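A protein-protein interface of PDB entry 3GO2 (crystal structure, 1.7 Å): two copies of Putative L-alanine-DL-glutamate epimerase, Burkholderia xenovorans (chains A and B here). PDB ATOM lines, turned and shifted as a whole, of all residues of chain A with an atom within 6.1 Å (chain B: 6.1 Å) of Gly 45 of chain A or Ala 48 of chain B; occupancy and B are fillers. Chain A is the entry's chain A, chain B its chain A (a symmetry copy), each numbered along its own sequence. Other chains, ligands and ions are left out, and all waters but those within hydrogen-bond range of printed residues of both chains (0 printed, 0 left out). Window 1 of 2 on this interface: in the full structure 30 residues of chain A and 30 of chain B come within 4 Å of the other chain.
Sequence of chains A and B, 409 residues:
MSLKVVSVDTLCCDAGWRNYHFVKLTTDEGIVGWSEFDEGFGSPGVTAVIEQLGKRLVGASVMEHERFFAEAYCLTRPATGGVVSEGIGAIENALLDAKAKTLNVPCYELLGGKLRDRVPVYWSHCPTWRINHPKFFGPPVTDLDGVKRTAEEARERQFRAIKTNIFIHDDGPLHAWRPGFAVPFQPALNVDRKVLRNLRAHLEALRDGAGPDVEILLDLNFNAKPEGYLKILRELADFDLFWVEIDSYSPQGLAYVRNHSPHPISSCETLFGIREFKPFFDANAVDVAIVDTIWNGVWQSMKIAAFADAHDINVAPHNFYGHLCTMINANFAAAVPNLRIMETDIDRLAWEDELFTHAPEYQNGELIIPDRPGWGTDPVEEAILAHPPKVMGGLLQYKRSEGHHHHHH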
ATOM      1  N   GLU A  39       9.420  29.733  -1.657  1.00  0.00           N
ATOM      2  CA  GLU A  39       8.329  28.912  -1.115  1.00  0.00           C
ATOM      3  C   GLU A  39       8.009  29.257   0.340  1.00  0.00           C
ATOM      4  O   GLU A  39       6.936  28.895   0.846  1.00  0.00           O
ATOM      5  CB  GLU A  39       8.667  27.438  -1.194  1.00  0.00           C
ATOM      6  CG  GLU A  39       8.703  26.908  -2.612  1.00  0.00           C
ATOM      7  CD  GLU A  39       8.886  25.430  -2.704  1.00  0.00           C
ATOM      8  OE1 GLU A  39       9.056  24.782  -1.657  1.00  0.00           O
ATOM      9  OE2 GLU A  39       8.863  24.913  -3.836  1.00  0.00           O
ATOM     10  N   SER A  43       4.032  29.660   0.459  1.00  0.00           N
ATOM     11  CA  SER A  43       3.935  29.159  -0.911  1.00  0.00           C
ATOM     12  C   SER A  43       4.552  27.768  -1.117  1.00  0.00           C
ATOM     13  O   SER A  43       5.386  27.578  -1.998  1.00  0.00           O
ATOM     14  CB  SER A  43       4.588  30.173  -1.867  1.00  0.00           C
ATOM     15  OG  SER A  43       3.999  31.453  -1.777  1.00  0.00           O
ATOM     16  N   PRO A  44       4.110  26.756  -0.342  1.00  0.00           N
ATOM     17  CA  PRO A  44       4.556  25.406  -0.642  1.00  0.00           C
ATOM     18  C   PRO A  44       4.097  24.943  -2.029  1.00  0.00           C
ATOM     19  O   PRO A  44       2.984  25.260  -2.436  1.00  0.00           O
ATOM     20  CB  PRO A  44       3.854  24.558   0.430  1.00  0.00           C
ATOM     21  CG  PRO A  44       2.628  25.354   0.803  1.00  0.00           C
ATOM     22  CD  PRO A  44       3.036  26.790   0.673  1.00  0.00           C
ATOM     23  N   GLY A  45       4.944  24.194  -2.731  1.00  0.00           N
ATOM     24  CA  GLY A  45       4.557  23.585  -3.998  1.00  0.00           C
ATOM     25  C   GLY A  45       5.055  24.263  -5.269  1.00  0.00           C
ATOM     26  O   GLY A  45       4.869  23.721  -6.379  1.00  0.00           O
ATOM     27  N   VAL A  46       5.663  25.452  -5.155  1.00  0.00           N
ATOM     28  CA  VAL A  46       6.103  26.166  -6.378  1.00  0.00           C
ATOM     29  C   VAL A  46       7.078  25.331  -7.216  1.00  0.00           C
ATOM     30  O   VAL A  46       6.972  25.258  -8.440  1.00  0.00           O
ATOM     31  CB  VAL A  46       6.748  27.548  -6.074  1.00  0.00           C
ATOM     32  CG1 VAL A  46       7.102  28.249  -7.374  1.00  0.00           C
ATOM     33  CG2 VAL A  46       5.771  28.413  -5.229  1.00  0.00           C
ATOM     34  N   THR A  47       8.028  24.684  -6.545  1.00  0.00           N
ATOM     35  CA  THR A  47       8.992  23.834  -7.247  1.00  0.00           C
ATOM     36  C   THR A  47       8.289  22.746  -8.055  1.00  0.00           C
ATOM     37  O   THR A  47       8.660  22.461  -9.194  1.00  0.00           O
ATOM     38  CB  THR A  47      10.023  23.211  -6.284  1.00  0.00           C
ATOM     39  OG1 THR A  47      10.693  24.241  -5.521  1.00  0.00           O
ATOM     40  CG2 THR A  47      11.039  22.353  -7.065  1.00  0.00           C
ATOM     41  N   ALA A  48       7.252  22.138  -7.480  1.00  0.00           N
ATOM     42  CA  ALA A  48       6.537  21.072  -8.173  1.00  0.00           C
ATOM     43  C   ALA A  48       5.839  21.565  -9.425  1.00  0.00           C
ATOM     44  O   ALA A  48       5.805  20.879 -10.445  1.00  0.00           O
ATOM     45  CB  ALA A  48       5.545  20.397  -7.230  1.00  0.00           C
ATOM     46  N   VAL A  49       5.249  22.755  -9.339  1.00  0.00           N
ATOM     47  CA  VAL A  49       4.650  23.408 -10.498  1.00  0.00           C
ATOM     48  C   VAL A  49       5.667  23.632 -11.608  1.00  0.00           C
ATOM     49  O   VAL A  49       5.434  23.304 -12.779  1.00  0.00           O
ATOM     50  CB  VAL A  49       3.991  24.784 -10.104  1.00  0.00           C
ATOM     51  CG1 VAL A  49       3.478  25.499 -11.344  1.00  0.00           C
ATOM     52  CG2 VAL A  49       2.868  24.559  -9.067  1.00  0.00           C
ATOM     53  N   ILE A  50       6.799  24.216 -11.241  1.00  0.00           N
ATOM     54  CA  ILE A  50       7.850  24.521 -12.214  1.00  0.00           C
ATOM     55  C   ILE A  50       8.359  23.253 -12.881  1.00  0.00           C
ATOM     56  O   ILE A  50       8.543  23.204 -14.095  1.00  0.00           O
ATOM     57  CB  ILE A  50       9.023  25.250 -11.535  1.00  0.00           C
ATOM     58  CG1 ILE A  50       8.567  26.642 -11.105  1.00  0.00           C
ATOM     59  CG2 ILE A  50      10.234  25.358 -12.491  1.00  0.00           C
ATOM     60  CD1 ILE A  50       9.493  27.290 -10.057  1.00  0.00           C
ATOM     61  N   VAL A  83       0.288  29.546  -6.053  1.00  0.00           N
ATOM     62  CA  VAL A  83       1.539  28.824  -6.301  1.00  0.00           C
ATOM     63  C   VAL A  83       1.700  28.409  -7.763  1.00  0.00           C
ATOM     64  O   VAL A  83       2.807  28.397  -8.265  1.00  0.00           O
ATOM     65  CB  VAL A  83       1.742  27.642  -5.336  1.00  0.00           C
ATOM     66  CG1 VAL A  83       1.962  28.120  -3.897  1.00  0.00           C
ATOM     67  CG2 VAL A  83       0.642  26.727  -5.381  1.00  0.00           C
ATOM     68  N   GLU B  39      -4.724  16.270  -9.325  1.00  0.00           N
ATOM     69  CA  GLU B  39      -3.739  17.209  -9.878  1.00  0.00           C
ATOM     70  C   GLU B  39      -3.904  17.403 -11.386  1.00  0.00           C
ATOM     71  O   GLU B  39      -3.378  18.375 -11.951  1.00  0.00           O
ATOM     72  CB  GLU B  39      -2.326  16.736  -9.609  1.00  0.00           C
ATOM     73  CG  GLU B  39      -1.943  16.798  -8.145  1.00  0.00           C
ATOM     74  CD  GLU B  39      -0.510  16.479  -7.878  1.00  0.00           C
ATOM     75  OE1 GLU B  39       0.213  16.134  -8.828  1.00  0.00           O
ATOM     76  OE2 GLU B  39      -0.105  16.572  -6.704  1.00  0.00           O
ATOM     77  N   PRO B  44      -1.064  21.082 -10.819  1.00  0.00           N
ATOM     78  CA  PRO B  44       0.193  20.538 -10.334  1.00  0.00           C
ATOM     79  C   PRO B  44       0.569  21.095  -8.957  1.00  0.00           C
ATOM     80  O   PRO B  44       0.338  22.271  -8.695  1.00  0.00           O
ATOM     81  CB  PRO B  44       1.213  21.032 -11.372  1.00  0.00           C
ATOM     82  CG  PRO B  44       0.599  22.284 -11.945  1.00  0.00           C
ATOM     83  CD  PRO B  44      -0.880  22.039 -11.931  1.00  0.00           C
ATOM     84  N   GLY B  45       1.147  20.257  -8.100  1.00  0.00           N
ATOM     85  CA  GLY B  45       1.670  20.715  -6.818  1.00  0.00           C
ATOM     86  C   GLY B  45       0.821  20.427  -5.584  1.00  0.00           C
ATOM     87  O   GLY B  45       1.271  20.675  -4.446  1.00  0.00           O
ATOM     88  N   VAL B  46      -0.411  19.933  -5.767  1.00  0.00           N
ATOM     89  CA  VAL B  46      -1.284  19.701  -4.590  1.00  0.00           C
ATOM     90  C   VAL B  46      -0.647  18.742  -3.577  1.00  0.00           C
ATOM     91  O   VAL B  46      -0.682  18.972  -2.369  1.00  0.00           O
ATOM     92  CB  VAL B  46      -2.694  19.169  -4.978  1.00  0.00           C
ATOM     93  CG1 VAL B  46      -3.552  19.028  -3.733  1.00  0.00           C
ATOM     94  CG2 VAL B  46      -3.359  20.131  -6.001  1.00  0.00           C
ATOM     95  N   THR B  47      -0.048  17.665  -4.080  1.00  0.00           N
ATOM     96  CA  THR B  47       0.618  16.702  -3.201  1.00  0.00           C
ATOM     97  C   THR B  47       1.694  17.375  -2.352  1.00  0.00           C
ATOM     98  O   THR B  47       1.825  17.102  -1.159  1.00  0.00           O
ATOM     99  CB  THR B  47       1.213  15.516  -3.987  1.00  0.00           C
ATOM    100  OG1 THR B  47       0.193  14.875  -4.788  1.00  0.00           O
ATOM    101  CG2 THR B  47       1.873  14.509  -3.023  1.00  0.00           C
ATOM    102  N   ALA B  48       2.466  18.278  -2.956  1.00  0.00           N
ATOM    103  CA  ALA B  48       3.533  18.953  -2.225  1.00  0.00           C
ATOM    104  C   ALA B  48       3.002  19.827  -1.106  1.00  0.00           C
ATOM    105  O   ALA B  48       3.585  19.902  -0.027  1.00  0.00           O
ATOM    106  CB  ALA B  48       4.402  19.764  -3.181  1.00  0.00           C
ATOM    107  N   VAL B  49       1.898  20.521  -1.376  1.00  0.00           N
ATOM    108  CA  VAL B  49       1.206  21.304  -0.358  1.00  0.00           C
ATOM    109  C   VAL B  49       0.766  20.440   0.815  1.00  0.00           C
ATOM    110  O   VAL B  49       1.002  20.763   1.986  1.00  0.00           O
ATOM    111  CB  VAL B  49      -0.043  22.051  -0.959  1.00  0.00           C
ATOM    112  CG1 VAL B  49      -0.813  22.764   0.141  1.00  0.00           C
ATOM    113  CG2 VAL B  49       0.404  23.028  -2.070  1.00  0.00           C
ATOM    114  N   ILE B  50       0.098  19.340   0.498  1.00  0.00           N
ATOM    115  CA  ILE B  50      -0.415  18.434   1.530  1.00  0.00           C
ATOM    116  C   ILE B  50       0.719  17.876   2.375  1.00  0.00           C
ATOM    117  O   ILE B  50       0.629  17.819   3.599  1.00  0.00           O
ATOM    118  CB  ILE B  50      -1.200  17.275   0.893  1.00  0.00           C
ATOM    119  CG1 ILE B  50      -2.485  17.820   0.274  1.00  0.00           C
ATOM    120  CG2 ILE B  50      -1.534  16.191   1.944  1.00  0.00           C
ATOM    121  CD1 ILE B  50      -3.128  16.856  -0.743  1.00  0.00           C
ATOM    122  N   GLU B  51       1.797  17.497   1.729  1.00  0.00           N
ATOM    123  CA  GLU B  51       2.945  16.967   2.483  1.00  0.00           C
ATOM    124  C   GLU B  51       3.498  17.955   3.500  1.00  0.00           C
ATOM    125  O   GLU B  51       3.876  17.557   4.595  1.00  0.00           O
ATOM    126  CB  GLU B  51       4.047  16.484   1.522  1.00  0.00           C
ATOM    127  CG  GLU B  51       3.698  15.160   0.819  1.00  0.00           C
ATOM    128  CD  GLU B  51       3.616  13.937   1.773  1.00  0.00           C
ATOM    129  OE1 GLU B  51       4.279  13.934   2.826  1.00  0.00           O
ATOM    130  OE2 GLU B  51       2.903  12.960   1.467  1.00  0.00           O
ATOM    131  N   GLN B  52       3.549  19.237   3.148  1.00  0.00           N
ATOM    132  CA  GLN B  52       4.008  20.287   4.088  1.00  0.00           C
ATOM    133  C   GLN B  52       2.985  20.546   5.181  1.00  0.00           C
ATOM    134  O   GLN B  52       3.309  20.584   6.366  1.00  0.00           O
ATOM    135  CB  GLN B  52       4.267  21.596   3.338  1.00  0.00           C
ATOM    136  CG  GLN B  52       5.487  21.539   2.519  1.00  0.00           C
ATOM    137  CD  GLN B  52       6.703  21.397   3.400  1.00  0.00           C
ATOM    138  OE1 GLN B  52       7.054  22.328   4.108  1.00  0.00           O
ATOM    139  NE2 GLN B  52       7.312  20.215   3.403  1.00  0.00           N
ATOM    140  N   LEU B  53       1.735  20.753   4.790  1.00  0.00           N
ATOM    141  CA  LEU B  53       0.684  21.028   5.767  1.00  0.00           C
ATOM    142  C   LEU B  53       0.405  19.874   6.720  1.00  0.00           C
ATOM    143  O   LEU B  53       0.123  20.093   7.909  1.00  0.00           O
ATOM    144  CB  LEU B  53      -0.614  21.448   5.062  1.00  0.00           C
ATOM    145  CG  LEU B  53      -0.549  22.851   4.477  1.00  0.00           C
ATOM    146  CD1 LEU B  53      -1.827  23.159   3.703  1.00  0.00           C
ATOM    147  CD2 LEU B  53      -0.329  23.897   5.592  1.00  0.00           C
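Pro 44 of chain A touches Val 49 of chain B (O to CG2, 3.4 Å).
Gly 45 of chain A touches Ala 48 of chain B (CA to CB, 3.9 Å).
CB of Ala 48 of chain A touches CA of Gly 45 of chain B, 3.9 Å away.
CG2 of Val 49 of chain A touches O of Pro 44 of chain B (3.4 Å).
Gly 45 of chain A touches one residue of chain B.
Of the printed residues of chain A, Ala 48 of chain B touches Gly 45 (3.9 Å).
Printed residues of chain B within 4 Å of Val 49 of chain A: Pro 44 (3.4 Å).
Of the printed residues of chain B, Ala 48 of chain A touches Gly 45.
Printed residues of chain A within 4 Å of Gly 45 of chain B: Ala 48.
Of the printed residues of chain A, Pro 44 of chain B touches Val 49.
Of the printed residues of chain A, Val 49 of chain B touches Pro 44 (3.4 Å).
Ser 43 of chain A touches none of the printed residues of chain B.
The nearest residue of chain A that does not touch Ala 48 of chain B is Ala 48 of chain A (4.3 Å).
Pro 44 of chain A touches Val 49 of chain B, and with the chains exchanged Val 49 of chain A touches Pro 44 of chain B.
Gly 45 of chain A touches Ala 48 of chain B, and with the chains exchanged Ala 48 of chain A touches Gly 45 of chain B.
Positions printed for both chains: 39, 44, 45, 46, 47, 48, 49 and 50.
Of the 4 pairs that touch across the chains among the printed residues, 4 have their exchanged pair printed and touching as well.
Of the 10 printed residues of chain A, 4 touch a printed residue of chain B.
Printed residues of chain B that touch a printed residue of chain A: Pro 44, Gly 45, Ala 48 and Val 49.
Hydrophobic or aromatic side chains of chain B within 4 Å of the printed part of chain A: Ala 48 and Val 49.
Among the printed residues, 4 pairs touch across the chains.
Among the printed residues, no Asp or Glu carboxylate lies within 4 Å of a Lys or Arg side-chain nitrogen of the other chain.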
